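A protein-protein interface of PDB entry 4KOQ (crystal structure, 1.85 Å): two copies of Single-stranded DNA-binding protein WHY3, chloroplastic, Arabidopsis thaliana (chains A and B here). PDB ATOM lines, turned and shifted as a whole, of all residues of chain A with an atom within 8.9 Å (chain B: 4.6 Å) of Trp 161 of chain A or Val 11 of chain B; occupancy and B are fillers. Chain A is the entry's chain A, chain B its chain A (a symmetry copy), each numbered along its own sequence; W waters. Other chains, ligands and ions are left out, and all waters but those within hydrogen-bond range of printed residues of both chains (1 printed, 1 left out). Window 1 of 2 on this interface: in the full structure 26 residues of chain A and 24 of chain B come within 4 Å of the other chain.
The backbone carbonyl oxygen of Phe 39 of chain A sits at hydrogen-bond distance from the backbone NH of Tyr 10 of chain B, 2.9 Å away.
The backbone carbonyl oxygen (O) of Val 11 of chain B lies within hydrogen-bond range of the indole nitrogen (NE1) of Trp 161 of chain A.
N of Leu 41 of chain A lies within hydrogen-bond range of O of Tyr 10 of chain B (3.0 Å).
N of Ser 162 of chain A is in hydrogen-bond range of O of Pro 156 of chain A (3.4 Å).
N of Val 11 of chain B is in hydrogen-bond range of OE2 of Glu 25 of chain B (3.0 Å).
OG of Ser 167 of chain A sits at hydrogen-bond distance from O of Phe 164 of chain A (2.7 Å).
The backbone carbonyl oxygen (O) of Ser 162 of chain A lies close to the side-chain amide nitrogen (ND2) of Asn 166 of chain A, at 3.2 Å.
ND1 of His 157 of chain A is in hydrogen-bond range of OG of Ser 162 of chain A (3.0 Å).
The backbone carbonyl oxygen (O) of His 13 of chain B sits at hydrogen-bond distance from the backbone NH (N) of Ile 24 of chain B, at 2.8 Å.
Among the printed residues, merely in contact across the chains: Pro 156 of chain A with Phe 153 of chain B (3.4 Å), Phe 39 of chain A with Phe 9 of chain B (3.4 Å), Gly 160 of chain A with Val 11 of chain B (3.5 Å), Phe 31 of chain A with Phe 9 of chain B (3.5 Å), Trp 161 of chain A with Ile 24 of chain B (3.6 Å), Ala 165 of chain A with Phe 153 of chain B (3.6 Å), Trp 161 of chain A with Pro 26 of chain B (3.6 Å), Trp 161 of chain A with Phe 153 of chain B (3.7 Å), Phe 164 of chain A with Pro 26 of chain B (3.7 Å), Glu 44 of chain A with His 13 of chain B (3.7 Å), Lys 40 of chain A with Tyr 10 of chain B (3.7 Å), Ile 159 of chain A with Val 11 of chain B (3.7 Å), Trp 161 of chain A with Ala 150 of chain B (3.8 Å), Phe 164 of chain A with Val 154 of chain B (3.8 Å), Ile 159 of chain A with Ala 150 of chain B (3.8 Å), Phe 31 of chain A with Val 11 of chain B (3.9 Å) and Ser 162 of chain A with Phe 153 of chain B (3.9 Å).
Of chain A, only Phe 31 (3.9 Å), Ile 159 (3.7 Å), Gly 160 (3.5 Å) and Trp 161 (2.9 Å) come within 4 Å of Val 11 of chain B.
Gly 12 of chain B touches none of the printed residues of chain A.
Of the printed residues of chain B, Ser 162 of chain A touches Phe 153 (3.9 Å).
Of the printed residues of chain B, Ile 159 of chain A touches Val 11 and Ala 150.
Of the printed residues of chain A, Ala 150 of chain B touches Ile 159 and Trp 161.
Glu 30 of chain A touches none of the printed residues of chain B.
Pro 29 of chain A touches none of the printed residues of chain B.
The nearest printed residue of chain B that does not touch Trp 161 of chain A is Leu 47 of chain B (4.01 Å).
The nearest residue of chain A that does not touch Val 11 of chain B is Leu 41 of chain A (4.2 Å).
Printed residues of chain B that touch a printed residue of chain A: Phe 9, Tyr 10, Val 11, His 13, Ile 24, Pro 26, Ala 150, Phe 153 and Val 154.
Of the 24 printed residues of chain A, 12 touch a printed residue of chain B.
Printed residues of chain A that touch a printed residue of chain B: Phe 31, Phe 39, Lys 40, Leu 41, Glu 44, Pro 156, Ile 159, Gly 160, Trp 161, Ser 162, Phe 164 and Ala 165.
Hydrophobic or aromatic side chains of chain A within 4 Å of the printed part of chain B: Phe 31, Phe 39, Leu 41, Pro 156, Ile 159, Trp 161, Phe 164 and Ala 165.
Among the printed residues, no Asp or Glu carboxylate lies within 4 Å of a Lys or Arg side-chain nitrogen of the other chain.
1 position is printed for both chains.
Water W1 lies within hydrogen-bond range of the side-chain carboxylate (OE2) of Glu 44 of chain A (2.5 Å) and a ring nitrogen (ND1) of His 13 of chain B (2.8 Å).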
ATOM      1  N   PRO A  29     -14.133  22.396  15.367  1.00  0.00           N
ATOM      2  CA  PRO A  29     -14.357  21.917  14.010  1.00  0.00           C
ATOM      3  C   PRO A  29     -14.806  20.442  13.998  1.00  0.00           C
ATOM      4  O   PRO A  29     -14.657  19.765  15.012  1.00  0.00           O
ATOM      5  CB  PRO A  29     -12.995  22.096  13.341  1.00  0.00           C
ATOM      6  CG  PRO A  29     -12.021  22.105  14.417  1.00  0.00           C
ATOM      7  CD  PRO A  29     -12.707  22.581  15.669  1.00  0.00           C
ATOM      8  N   GLU A  30     -15.356  19.998  12.868  1.00  0.00           N
ATOM      9  CA  GLU A  30     -15.764  18.610  12.681  1.00  0.00           C
ATOM     10  C   GLU A  30     -14.826  17.938  11.699  1.00  0.00           C
ATOM     11  O   GLU A  30     -14.371  18.551  10.737  1.00  0.00           O
ATOM     12  CB  GLU A  30     -17.195  18.524  12.165  1.00  0.00           C
ATOM     13  CG  GLU A  30     -18.231  18.937  13.177  1.00  0.00           C
ATOM     14  CD  GLU A  30     -19.651  18.882  12.622  1.00  0.00           C
ATOM     15  OE1 GLU A  30     -19.832  18.397  11.485  1.00  0.00           O
ATOM     16  OE2 GLU A  30     -20.588  19.328  13.319  1.00  0.00           O
ATOM     17  N   PHE A  31     -14.534  16.669  11.973  1.00  0.00           N
ATOM     18  CA  PHE A  31     -13.615  15.891  11.171  1.00  0.00           C
ATOM     19  C   PHE A  31     -14.314  14.613  10.721  1.00  0.00           C
ATOM     20  O   PHE A  31     -15.305  14.200  11.319  1.00  0.00           O
ATOM     21  CB  PHE A  31     -12.403  15.518  12.014  1.00  0.00           C
ATOM     22  CG  PHE A  31     -11.499  16.659  12.299  1.00  0.00           C
ATOM     23  CD1 PHE A  31     -10.520  17.001  11.400  1.00  0.00           C
ATOM     24  CD2 PHE A  31     -11.633  17.402  13.453  1.00  0.00           C
ATOM     25  CE1 PHE A  31      -9.682  18.041  11.644  1.00  0.00           C
ATOM     26  CE2 PHE A  31     -10.784  18.453  13.702  1.00  0.00           C
ATOM     27  CZ  PHE A  31      -9.816  18.774  12.789  1.00  0.00           C
ATOM     28  N   PHE A  39      -7.474  12.050   9.261  1.00  0.00           N
ATOM     29  CA  PHE A  39      -8.745  12.736   9.443  1.00  0.00           C
ATOM     30  C   PHE A  39      -8.785  13.988   8.581  1.00  0.00           C
ATOM     31  O   PHE A  39      -7.761  14.618   8.323  1.00  0.00           O
ATOM     32  CB  PHE A  39      -8.933  13.097  10.904  1.00  0.00           C
ATOM     33  CG  PHE A  39      -9.022  11.916  11.793  1.00  0.00           C
ATOM     34  CD1 PHE A  39     -10.217  11.237  11.941  1.00  0.00           C
ATOM     35  CD2 PHE A  39      -7.908  11.468  12.480  1.00  0.00           C
ATOM     36  CE1 PHE A  39     -10.300  10.135  12.771  1.00  0.00           C
ATOM     37  CE2 PHE A  39      -7.987  10.369  13.308  1.00  0.00           C
ATOM     38  CZ  PHE A  39      -9.182   9.703  13.454  1.00  0.00           C
ATOM     39  N   LYS A  40      -9.970  14.323   8.105  1.00  0.00           N
ATOM     40  CA  LYS A  40     -10.125  15.475   7.245  1.00  0.00           C
ATOM     41  C   LYS A  40     -11.128  16.413   7.881  1.00  0.00           C
ATOM     42  O   LYS A  40     -12.195  15.977   8.315  1.00  0.00           O
ATOM     43  CB  LYS A  40     -10.646  15.058   5.890  1.00  0.00           C
ATOM     44  CG  LYS A  40     -10.874  16.209   4.939  1.00  0.00           C
ATOM     45  CD  LYS A  40     -11.676  15.752   3.731  1.00  0.00           C
ATOM     46  CE  LYS A  40     -11.456  16.660   2.530  1.00  0.00           C
ATOM     47  NZ  LYS A  40     -10.082  16.516   1.960  1.00  0.00           N
ATOM     48  N   LEU A  41     -10.794  17.697   7.898  1.00  0.00           N
ATOM     49  CA  LEU A  41     -11.676  18.702   8.476  1.00  0.00           C
ATOM     50  C   LEU A  41     -12.810  18.892   7.523  1.00  0.00           C
ATOM     51  O   LEU A  41     -12.584  19.221   6.378  1.00  0.00           O
ATOM     52  CB  LEU A  41     -10.924  20.044   8.684  1.00  0.00           C
ATOM     53  CG  LEU A  41     -11.836  21.147   9.262  1.00  0.00           C
ATOM     54  CD1 LEU A  41     -11.056  22.025  10.222  1.00  0.00           C
ATOM     55  CD2 LEU A  41     -12.385  21.978   8.161  1.00  0.00           C
ATOM     56  N   THR A  42     -14.036  18.691   7.988  1.00  0.00           N
ATOM     57  CA  THR A  42     -15.197  18.808   7.129  1.00  0.00           C
ATOM     58  C   THR A  42     -16.062  20.027   7.465  1.00  0.00           C
ATOM     59  O   THR A  42     -16.877  20.454   6.656  1.00  0.00           O
ATOM     60  CB  THR A  42     -16.073  17.564   7.247  1.00  0.00           C
ATOM     61  OG1 THR A  42     -16.386  17.333   8.624  1.00  0.00           O
ATOM     62  CG2 THR A  42     -15.335  16.344   6.678  1.00  0.00           C
ATOM     63  N   LYS A  43     -15.894  20.580   8.664  1.00  0.00           N
ATOM     64  CA  LYS A  43     -16.586  21.816   9.029  1.00  0.00           C
ATOM     65  C   LYS A  43     -15.728  22.631  10.009  1.00  0.00           C
ATOM     66  O   LYS A  43     -15.269  22.104  10.991  1.00  0.00           O
ATOM     67  CB  LYS A  43     -17.925  21.493   9.677  1.00  0.00           C
ATOM     68  CG  LYS A  43     -18.833  22.705   9.884  1.00  0.00           C
ATOM     69  CD  LYS A  43     -20.087  22.321  10.643  1.00  0.00           C
ATOM     70  CE  LYS A  43     -21.230  23.304  10.412  1.00  0.00           C
ATOM     71  NZ  LYS A  43     -21.029  24.596  11.111  1.00  0.00           N
ATOM     72  N   GLU A  44     -15.492  23.894   9.684  1.00  0.00           N
ATOM     73  CA  GLU A  44     -14.797  24.789  10.585  1.00  0.00           C
ATOM     74  C   GLU A  44     -15.539  24.897  11.886  1.00  0.00           C
ATOM     75  O   GLU A  44     -16.763  24.743  11.965  1.00  0.00           O
ATOM     76  CB  GLU A  44     -14.728  26.188  10.004  1.00  0.00           C
ATOM     77  CG  GLU A  44     -13.951  26.357   8.785  1.00  0.00           C
ATOM     78  CD  GLU A  44     -13.975  27.807   8.347  1.00  0.00           C
ATOM     79  OE1 GLU A  44     -15.069  28.466   8.445  1.00  0.00           O
ATOM     80  OE2 GLU A  44     -12.882  28.283   7.957  1.00  0.00           O
ATOM     81  N   VAL A 154      -8.493  31.817  19.361  1.00  0.00           N
ATOM     82  CA  VAL A 154      -9.304  30.668  19.003  1.00  0.00           C
ATOM     83  C   VAL A 154      -9.306  30.392  17.509  1.00  0.00           C
ATOM     84  O   VAL A 154      -9.540  29.263  17.091  1.00  0.00           O
ATOM     85  CB  VAL A 154     -10.740  30.806  19.572  1.00  0.00           C
ATOM     86  CG1 VAL A 154     -11.591  31.667  18.701  1.00  0.00           C
ATOM     87  CG2 VAL A 154     -11.331  29.436  19.789  1.00  0.00           C
ATOM     88  N   LEU A 155      -9.023  31.399  16.705  1.00  0.00           N
ATOM     89  CA  LEU A 155      -9.121  31.228  15.268  1.00  0.00           C
ATOM     90  C   LEU A 155      -8.320  30.030  14.705  1.00  0.00           C
ATOM     91  O   LEU A 155      -8.858  29.250  13.929  1.00  0.00           O
ATOM     92  CB  LEU A 155      -8.759  32.524  14.549  1.00  0.00           C
ATOM     93  CG  LEU A 155      -9.862  33.555  14.284  1.00  0.00           C
ATOM     94  CD1 LEU A 155      -9.256  34.875  13.826  1.00  0.00           C
ATOM     95  CD2 LEU A 155     -10.851  33.106  13.266  1.00  0.00           C
ATOM     96  N   PRO A 156      -7.041  29.881  15.099  1.00  0.00           N
ATOM     97  CA  PRO A 156      -6.257  28.712  14.623  1.00  0.00           C
ATOM     98  C   PRO A 156      -6.818  27.360  15.023  1.00  0.00           C
ATOM     99  O   PRO A 156      -6.692  26.397  14.256  1.00  0.00           O
ATOM    100  CB  PRO A 156      -4.860  28.942  15.200  1.00  0.00           C
ATOM    101  CG  PRO A 156      -4.937  30.142  16.010  1.00  0.00           C
ATOM    102  CD  PRO A 156      -6.209  30.850  15.824  1.00  0.00           C
ATOM    103  N   HIS A 157      -7.501  27.293  16.157  1.00  0.00           N
ATOM    104  CA  HIS A 157      -8.192  26.081  16.563  1.00  0.00           C
ATOM    105  C   HIS A 157      -9.417  25.833  15.754  1.00  0.00           C
ATOM    106  O   HIS A 157      -9.691  24.689  15.393  1.00  0.00           O
ATOM    107  CB  HIS A 157      -8.557  26.190  18.047  1.00  0.00           C
ATOM    108  CG  HIS A 157      -7.360  26.358  18.916  1.00  0.00           C
ATOM    109  ND1 HIS A 157      -6.682  25.286  19.455  1.00  0.00           N
ATOM    110  CD2 HIS A 157      -6.691  27.469  19.310  1.00  0.00           C
ATOM    111  CE1 HIS A 157      -5.643  25.731  20.144  1.00  0.00           C
ATOM    112  NE2 HIS A 157      -5.616  27.050  20.059  1.00  0.00           N
ATOM    113  N   LEU A 158     -10.166  26.893  15.428  1.00  0.00           N
ATOM    114  CA  LEU A 158     -11.390  26.714  14.679  1.00  0.00           C
ATOM    115  C   LEU A 158     -11.152  26.224  13.257  1.00  0.00           C
ATOM    116  O   LEU A 158     -12.048  25.562  12.673  1.00  0.00           O
ATOM    117  CB  LEU A 158     -12.270  27.965  14.639  1.00  0.00           C
ATOM    118  CG  LEU A 158     -12.659  28.559  15.992  1.00  0.00           C
ATOM    119  CD1 LEU A 158     -13.541  29.784  15.812  1.00  0.00           C
ATOM    120  CD2 LEU A 158     -13.303  27.590  16.931  1.00  0.00           C
ATOM    121  N   ILE A 159      -9.996  26.563  12.701  1.00  0.00           N
ATOM    122  CA  ILE A 159      -9.651  26.126  11.349  1.00  0.00           C
ATOM    123  C   ILE A 159      -8.824  24.825  11.341  1.00  0.00           C
ATOM    124  O   ILE A 159      -8.393  24.364  10.287  1.00  0.00           O
ATOM    125  CB  ILE A 159      -8.939  27.205  10.550  1.00  0.00           C
ATOM    126  CG1 ILE A 159      -7.577  27.523  11.137  1.00  0.00           C
ATOM    127  CG2 ILE A 159      -9.800  28.472  10.505  1.00  0.00           C
ATOM    128  CD1 ILE A 159      -6.718  28.486  10.270  1.00  0.00           C
ATOM    129  N   GLY A 160      -8.609  24.253  12.510  1.00  0.00           N
ATOM    130  CA  GLY A 160      -7.910  22.986  12.649  1.00  0.00           C
ATOM    131  C   GLY A 160      -6.410  23.016  12.651  1.00  0.00           C
ATOM    132  O   GLY A 160      -5.789  21.954  12.637  1.00  0.00           O
ATOM    133  N   TRP A 161      -5.806  24.202  12.693  1.00  0.00           N
ATOM    134  CA  TRP A 161      -4.374  24.300  12.592  1.00  0.00           C
ATOM    135  C   TRP A 161      -3.689  23.957  13.901  1.00  0.00           C
ATOM    136  O   TRP A 161      -2.504  23.710  13.921  1.00  0.00           O
ATOM    137  CB  TRP A 161      -3.931  25.676  12.084  1.00  0.00           C
ATOM    138  CG  TRP A 161      -4.148  25.837  10.596  1.00  0.00           C
ATOM    139  CD1 TRP A 161      -4.967  25.111   9.804  1.00  0.00           C
ATOM    140  CD2 TRP A 161      -3.481  26.758   9.743  1.00  0.00           C
ATOM    141  NE1 TRP A 161      -4.897  25.561   8.498  1.00  0.00           N
ATOM    142  CE2 TRP A 161      -3.982  26.571   8.443  1.00  0.00           C
ATOM    143  CE3 TRP A 161      -2.540  27.747   9.958  1.00  0.00           C
ATOM    144  CZ2 TRP A 161      -3.541  27.318   7.371  1.00  0.00           C
ATOM    145  CZ3 TRP A 161      -2.104  28.493   8.889  1.00  0.00           C
ATOM    146  CH2 TRP A 161      -2.593  28.258   7.609  1.00  0.00           C
ATOM    147  N   SER A 162      -4.428  23.906  15.000  1.00  0.00           N
ATOM    148  CA  SER A 162      -3.800  23.555  16.273  1.00  0.00           C
ATOM    149  C   SER A 162      -3.536  22.085  16.241  1.00  0.00           C
ATOM    150  O   SER A 162      -2.556  21.615  16.802  1.00  0.00           O
ATOM    151  CB  SER A 162      -4.696  23.893  17.459  1.00  0.00           C
ATOM    152  OG  SER A 162      -6.006  23.397  17.251  1.00  0.00           O
ATOM    153  N   ALA A 163      -4.446  21.365  15.614  1.00  0.00           N
ATOM    154  CA  ALA A 163      -4.281  19.952  15.372  1.00  0.00           C
ATOM    155  C   ALA A 163      -2.944  19.709  14.634  1.00  0.00           C
ATOM    156  O   ALA A 163      -2.209  18.774  14.961  1.00  0.00           O
ATOM    157  CB  ALA A 163      -5.456  19.445  14.575  1.00  0.00           C
ATOM    158  N   PHE A 164      -2.615  20.573  13.663  1.00  0.00           N
ATOM    159  CA  PHE A 164      -1.342  20.469  12.936  1.00  0.00           C
ATOM    160  C   PHE A 164      -0.204  20.827  13.857  1.00  0.00           C
ATOM    161  O   PHE A 164       0.817  20.133  13.926  1.00  0.00           O
ATOM    162  CB  PHE A 164      -1.331  21.402  11.694  1.00  0.00           C
ATOM    163  CG  PHE A 164       0.058  21.827  11.230  1.00  0.00           C
ATOM    164  CD1 PHE A 164       0.787  21.048  10.307  1.00  0.00           C
ATOM    165  CD2 PHE A 164       0.617  23.026  11.674  1.00  0.00           C
ATOM    166  CE1 PHE A 164       2.061  21.461   9.869  1.00  0.00           C
ATOM    167  CE2 PHE A 164       1.903  23.439  11.238  1.00  0.00           C
ATOM    168  CZ  PHE A 164       2.616  22.646  10.336  1.00  0.00           C
ATOM    169  N   ALA A 165      -0.382  21.928  14.569  1.00  0.00           N
ATOM    170  CA  ALA A 165       0.664  22.454  15.453  1.00  0.00           C
ATOM    171  C   ALA A 165       1.147  21.474  16.517  1.00  0.00           C
ATOM    172  O   ALA A 165       2.353  21.246  16.682  1.00  0.00           O
ATOM    173  CB  ALA A 165       0.161  23.691  16.139  1.00  0.00           C
ATOM    174  N   ASN A 166       0.217  20.934  17.284  1.00  0.00           N
ATOM    175  CA  ASN A 166       0.607  20.062  18.382  1.00  0.00           C
ATOM    176  C   ASN A 166       0.901  18.638  17.911  1.00  0.00           C
ATOM    177  O   ASN A 166       1.209  17.771  18.724  1.00  0.00           O
ATOM    178  CB  ASN A 166      -0.445  20.083  19.492  1.00  0.00           C
ATOM    179  CG  ASN A 166      -1.784  19.603  19.021  1.00  0.00           C
ATOM    180  OD1 ASN A 166      -1.865  18.762  18.128  1.00  0.00           O
ATOM    181  ND2 ASN A 166      -2.855  20.141  19.612  1.00  0.00           N
ATOM    182  N   SER A 167       0.835  18.412  16.598  1.00  0.00           N
ATOM    183  CA  SER A 167       1.198  17.120  16.023  1.00  0.00           C
ATOM    184  C   SER A 167       2.662  17.086  15.568  1.00  0.00           C
ATOM    185  O   SER A 167       3.219  16.014  15.328  1.00  0.00           O
ATOM    186  CB  SER A 167       0.291  16.774  14.837  1.00  0.00           C
ATOM    187  OG  SER A 167       0.696  17.449  13.653  1.00  0.00           O
ATOM    188  N   ILE A 168       3.285  18.257  15.449  1.00  0.00           N
ATOM    189  CA  ILE A 168       4.661  18.337  14.972  1.00  0.00           C
ATOM    190  C   ILE A 168       5.608  17.621  15.929  1.00  0.00           C
ATOM    191  O   ILE A 168       6.491  16.882  15.495  1.00  0.00           O
ATOM    192  CB  ILE A 168       5.127  19.797  14.815  1.00  0.00           C
ATOM    193  CG1 ILE A 168       4.292  20.521  13.755  1.00  0.00           C
ATOM    194  CG2 ILE A 168       6.606  19.848  14.434  1.00  0.00           C
ATOM    195  CD1 ILE A 168       4.646  21.977  13.604  1.00  0.00           C
ATOM    196  N   PHE B   9      -3.653  14.836   9.575  1.00  0.00           N
ATOM    197  CA  PHE B   9      -4.787  15.766   9.579  1.00  0.00           C
ATOM    198  C   PHE B   9      -4.752  16.685   8.345  1.00  0.00           C
ATOM    199  O   PHE B   9      -3.785  17.408   8.116  1.00  0.00           O
ATOM    200  CB  PHE B   9      -4.789  16.610  10.866  1.00  0.00           C
ATOM    201  CG  PHE B   9      -5.491  15.956  12.034  1.00  0.00           C
ATOM    202  CD1 PHE B   9      -6.867  16.037  12.172  1.00  0.00           C
ATOM    203  CD2 PHE B   9      -4.773  15.269  13.002  1.00  0.00           C
ATOM    204  CE1 PHE B   9      -7.518  15.437  13.250  1.00  0.00           C
ATOM    205  CE2 PHE B   9      -5.419  14.669  14.075  1.00  0.00           C
ATOM    206  CZ  PHE B   9      -6.794  14.753  14.197  1.00  0.00           C
ATOM    207  N   TYR B  10      -5.813  16.638   7.550  1.00  0.00           N
ATOM    208  CA  TYR B  10      -5.981  17.531   6.416  1.00  0.00           C
ATOM    209  C   TYR B  10      -6.828  18.703   6.876  1.00  0.00           C
ATOM    210  O   TYR B  10      -8.036  18.548   7.109  1.00  0.00           O
ATOM    211  CB  TYR B  10      -6.716  16.834   5.284  1.00  0.00           C
ATOM    212  CG  TYR B  10      -5.885  15.791   4.578  1.00  0.00           C
ATOM    213  CD1 TYR B  10      -4.920  16.162   3.655  1.00  0.00           C
ATOM    214  CD2 TYR B  10      -6.073  14.438   4.823  1.00  0.00           C
ATOM    215  CE1 TYR B  10      -4.163  15.228   2.996  1.00  0.00           C
ATOM    216  CE2 TYR B  10      -5.307  13.484   4.163  1.00  0.00           C
ATOM    217  CZ  TYR B  10      -4.355  13.895   3.252  1.00  0.00           C
ATOM    218  OH  TYR B  10      -3.587  12.971   2.573  1.00  0.00           O
ATOM    219  N   VAL B  11      -6.193  19.861   6.973  1.00  0.00           N
ATOM    220  CA  VAL B  11      -6.849  21.033   7.570  1.00  0.00           C
ATOM    221  C   VAL B  11      -6.603  22.289   6.730  1.00  0.00           C
ATOM    222  O   VAL B  11      -6.413  23.387   7.262  1.00  0.00           O
ATOM    223  CB  VAL B  11      -6.359  21.244   9.032  1.00  0.00           C
ATOM    224  CG1 VAL B  11      -6.869  20.087   9.939  1.00  0.00           C
ATOM    225  CG2 VAL B  11      -4.864  21.353   9.105  1.00  0.00           C
ATOM    226  N   GLY B  12      -6.616  22.130   5.407  1.00  0.00           N
ATOM    227  CA  GLY B  12      -6.536  23.270   4.514  1.00  0.00           C
ATOM    228  C   GLY B  12      -7.597  24.316   4.830  1.00  0.00           C
ATOM    229  O   GLY B  12      -8.741  24.010   5.130  1.00  0.00           O
ATOM    230  N   HIS B  13      -7.183  25.570   4.814  1.00  0.00           N
ATOM    231  CA  HIS B  13      -8.106  26.662   4.992  1.00  0.00           C
ATOM    232  C   HIS B  13      -8.405  27.224   3.610  1.00  0.00           C
ATOM    233  O   HIS B  13      -7.500  27.613   2.898  1.00  0.00           O
ATOM    234  CB  HIS B  13      -7.502  27.701   5.927  1.00  0.00           C
ATOM    235  CG  HIS B  13      -8.276  28.981   5.999  1.00  0.00           C
ATOM    236  ND1 HIS B  13      -9.541  29.068   6.551  1.00  0.00           N
ATOM    237  CD2 HIS B  13      -7.967  30.220   5.564  1.00  0.00           C
ATOM    238  CE1 HIS B  13      -9.968  30.316   6.457  1.00  0.00           C
ATOM    239  NE2 HIS B  13      -9.037  31.033   5.853  1.00  0.00           N
ATOM    240  N   ILE B  24      -5.053  26.929   1.615  1.00  0.00           N
ATOM    241  CA  ILE B  24      -3.776  27.125   2.286  1.00  0.00           C
ATOM    242  C   ILE B  24      -3.580  26.034   3.319  1.00  0.00           C
ATOM    243  O   ILE B  24      -4.394  25.887   4.236  1.00  0.00           O
ATOM    244  CB  ILE B  24      -3.733  28.478   3.011  1.00  0.00           C
ATOM    245  CG1 ILE B  24      -4.035  29.582   1.995  1.00  0.00           C
ATOM    246  CG2 ILE B  24      -2.394  28.718   3.655  1.00  0.00           C
ATOM    247  CD1 ILE B  24      -4.149  30.946   2.580  1.00  0.00           C
ATOM    248  N   GLU B  25      -2.507  25.276   3.144  1.00  0.00           N
ATOM    249  CA  GLU B  25      -2.201  24.122   4.010  1.00  0.00           C
ATOM    250  C   GLU B  25      -0.838  24.238   4.664  1.00  0.00           C
ATOM    251  O   GLU B  25       0.170  24.438   4.010  1.00  0.00           O
ATOM    252  CB  GLU B  25      -2.235  22.797   3.228  1.00  0.00           C
ATOM    253  CG  GLU B  25      -2.033  21.572   4.156  1.00  0.00           C
ATOM    254  CD  GLU B  25      -3.279  20.690   4.388  1.00  0.00           C
ATOM    255  OE1 GLU B  25      -4.002  20.427   3.395  1.00  0.00           O
ATOM    256  OE2 GLU B  25      -3.520  20.245   5.561  1.00  0.00           O
ATOM    257  N   PRO B  26      -0.787  24.075   5.977  1.00  0.00           N
ATOM    258  CA  PRO B  26       0.541  24.121   6.576  1.00  0.00           C
ATOM    259  C   PRO B  26       1.330  22.824   6.354  1.00  0.00           C
ATOM    260  O   PRO B  26       0.760  21.736   6.188  1.00  0.00           O
ATOM    261  CB  PRO B  26       0.250  24.362   8.053  1.00  0.00           C
ATOM    262  CG  PRO B  26      -1.151  24.073   8.235  1.00  0.00           C
ATOM    263  CD  PRO B  26      -1.859  24.003   6.973  1.00  0.00           C
ATOM    264  N   LEU B  47       3.965  27.207   4.131  1.00  0.00           N
ATOM    265  CA  LEU B  47       2.570  27.092   3.792  1.00  0.00           C
ATOM    266  C   LEU B  47       2.437  26.824   2.300  1.00  0.00           C
ATOM    267  O   LEU B  47       3.065  27.503   1.467  1.00  0.00           O
ATOM    268  CB  LEU B  47       1.818  28.414   4.096  1.00  0.00           C
ATOM    269  CG  LEU B  47       1.761  28.800   5.580  1.00  0.00           C
ATOM    270  CD1 LEU B  47       0.971  30.074   5.806  1.00  0.00           C
ATOM    271  CD2 LEU B  47       1.205  27.699   6.453  1.00  0.00           C
ATOM    272  N   ALA B 150      -3.910  33.387  11.618  1.00  0.00           N
ATOM    273  CA  ALA B 150      -3.430  32.034  11.400  1.00  0.00           C
ATOM    274  C   ALA B 150      -1.921  32.020  11.116  1.00  0.00           C
ATOM    275  O   ALA B 150      -1.218  31.125  11.573  1.00  0.00           O
ATOM    276  CB  ALA B 150      -4.183  31.380  10.230  1.00  0.00           C
ATOM    277  N   PHE B 153      -0.003  32.728  14.290  1.00  0.00           N
ATOM    278  CA  PHE B 153      -0.066  31.486  15.041  1.00  0.00           C
ATOM    279  C   PHE B 153       0.968  30.459  14.564  1.00  0.00           C
ATOM    280  O   PHE B 153       1.651  29.793  15.367  1.00  0.00           O
ATOM    281  CB  PHE B 153      -1.462  30.884  14.975  1.00  0.00           C
ATOM    282  CG  PHE B 153      -1.522  29.458  15.389  1.00  0.00           C
ATOM    283  CD1 PHE B 153      -1.623  29.128  16.740  1.00  0.00           C
ATOM    284  CD2 PHE B 153      -1.465  28.436  14.468  1.00  0.00           C
ATOM    285  CE1 PHE B 153      -1.661  27.822  17.134  1.00  0.00           C
ATOM    286  CE2 PHE B 153      -1.500  27.108  14.885  1.00  0.00           C
ATOM    287  CZ  PHE B 153      -1.591  26.812  16.217  1.00  0.00           C
ATOM    288  N   VAL B 154       1.059  30.283  13.256  1.00  0.00           N
ATOM    289  CA  VAL B 154       1.782  29.143  12.726  1.00  0.00           C
ATOM    290  C   VAL B 154       3.281  29.378  12.657  1.00  0.00           C
ATOM    291  O   VAL B 154       4.056  28.427  12.673  1.00  0.00           O
ATOM    292  CB  VAL B 154       1.197  28.705  11.358  1.00  0.00           C
ATOM    293  CG1 VAL B 154       1.725  29.546  10.245  1.00  0.00           C
ATOM    294  CG2 VAL B 154       1.455  27.235  11.146  1.00  0.00           C
HETATM  295  O   HOH W   1     -10.957  26.853   7.419  1.00  0.00           O
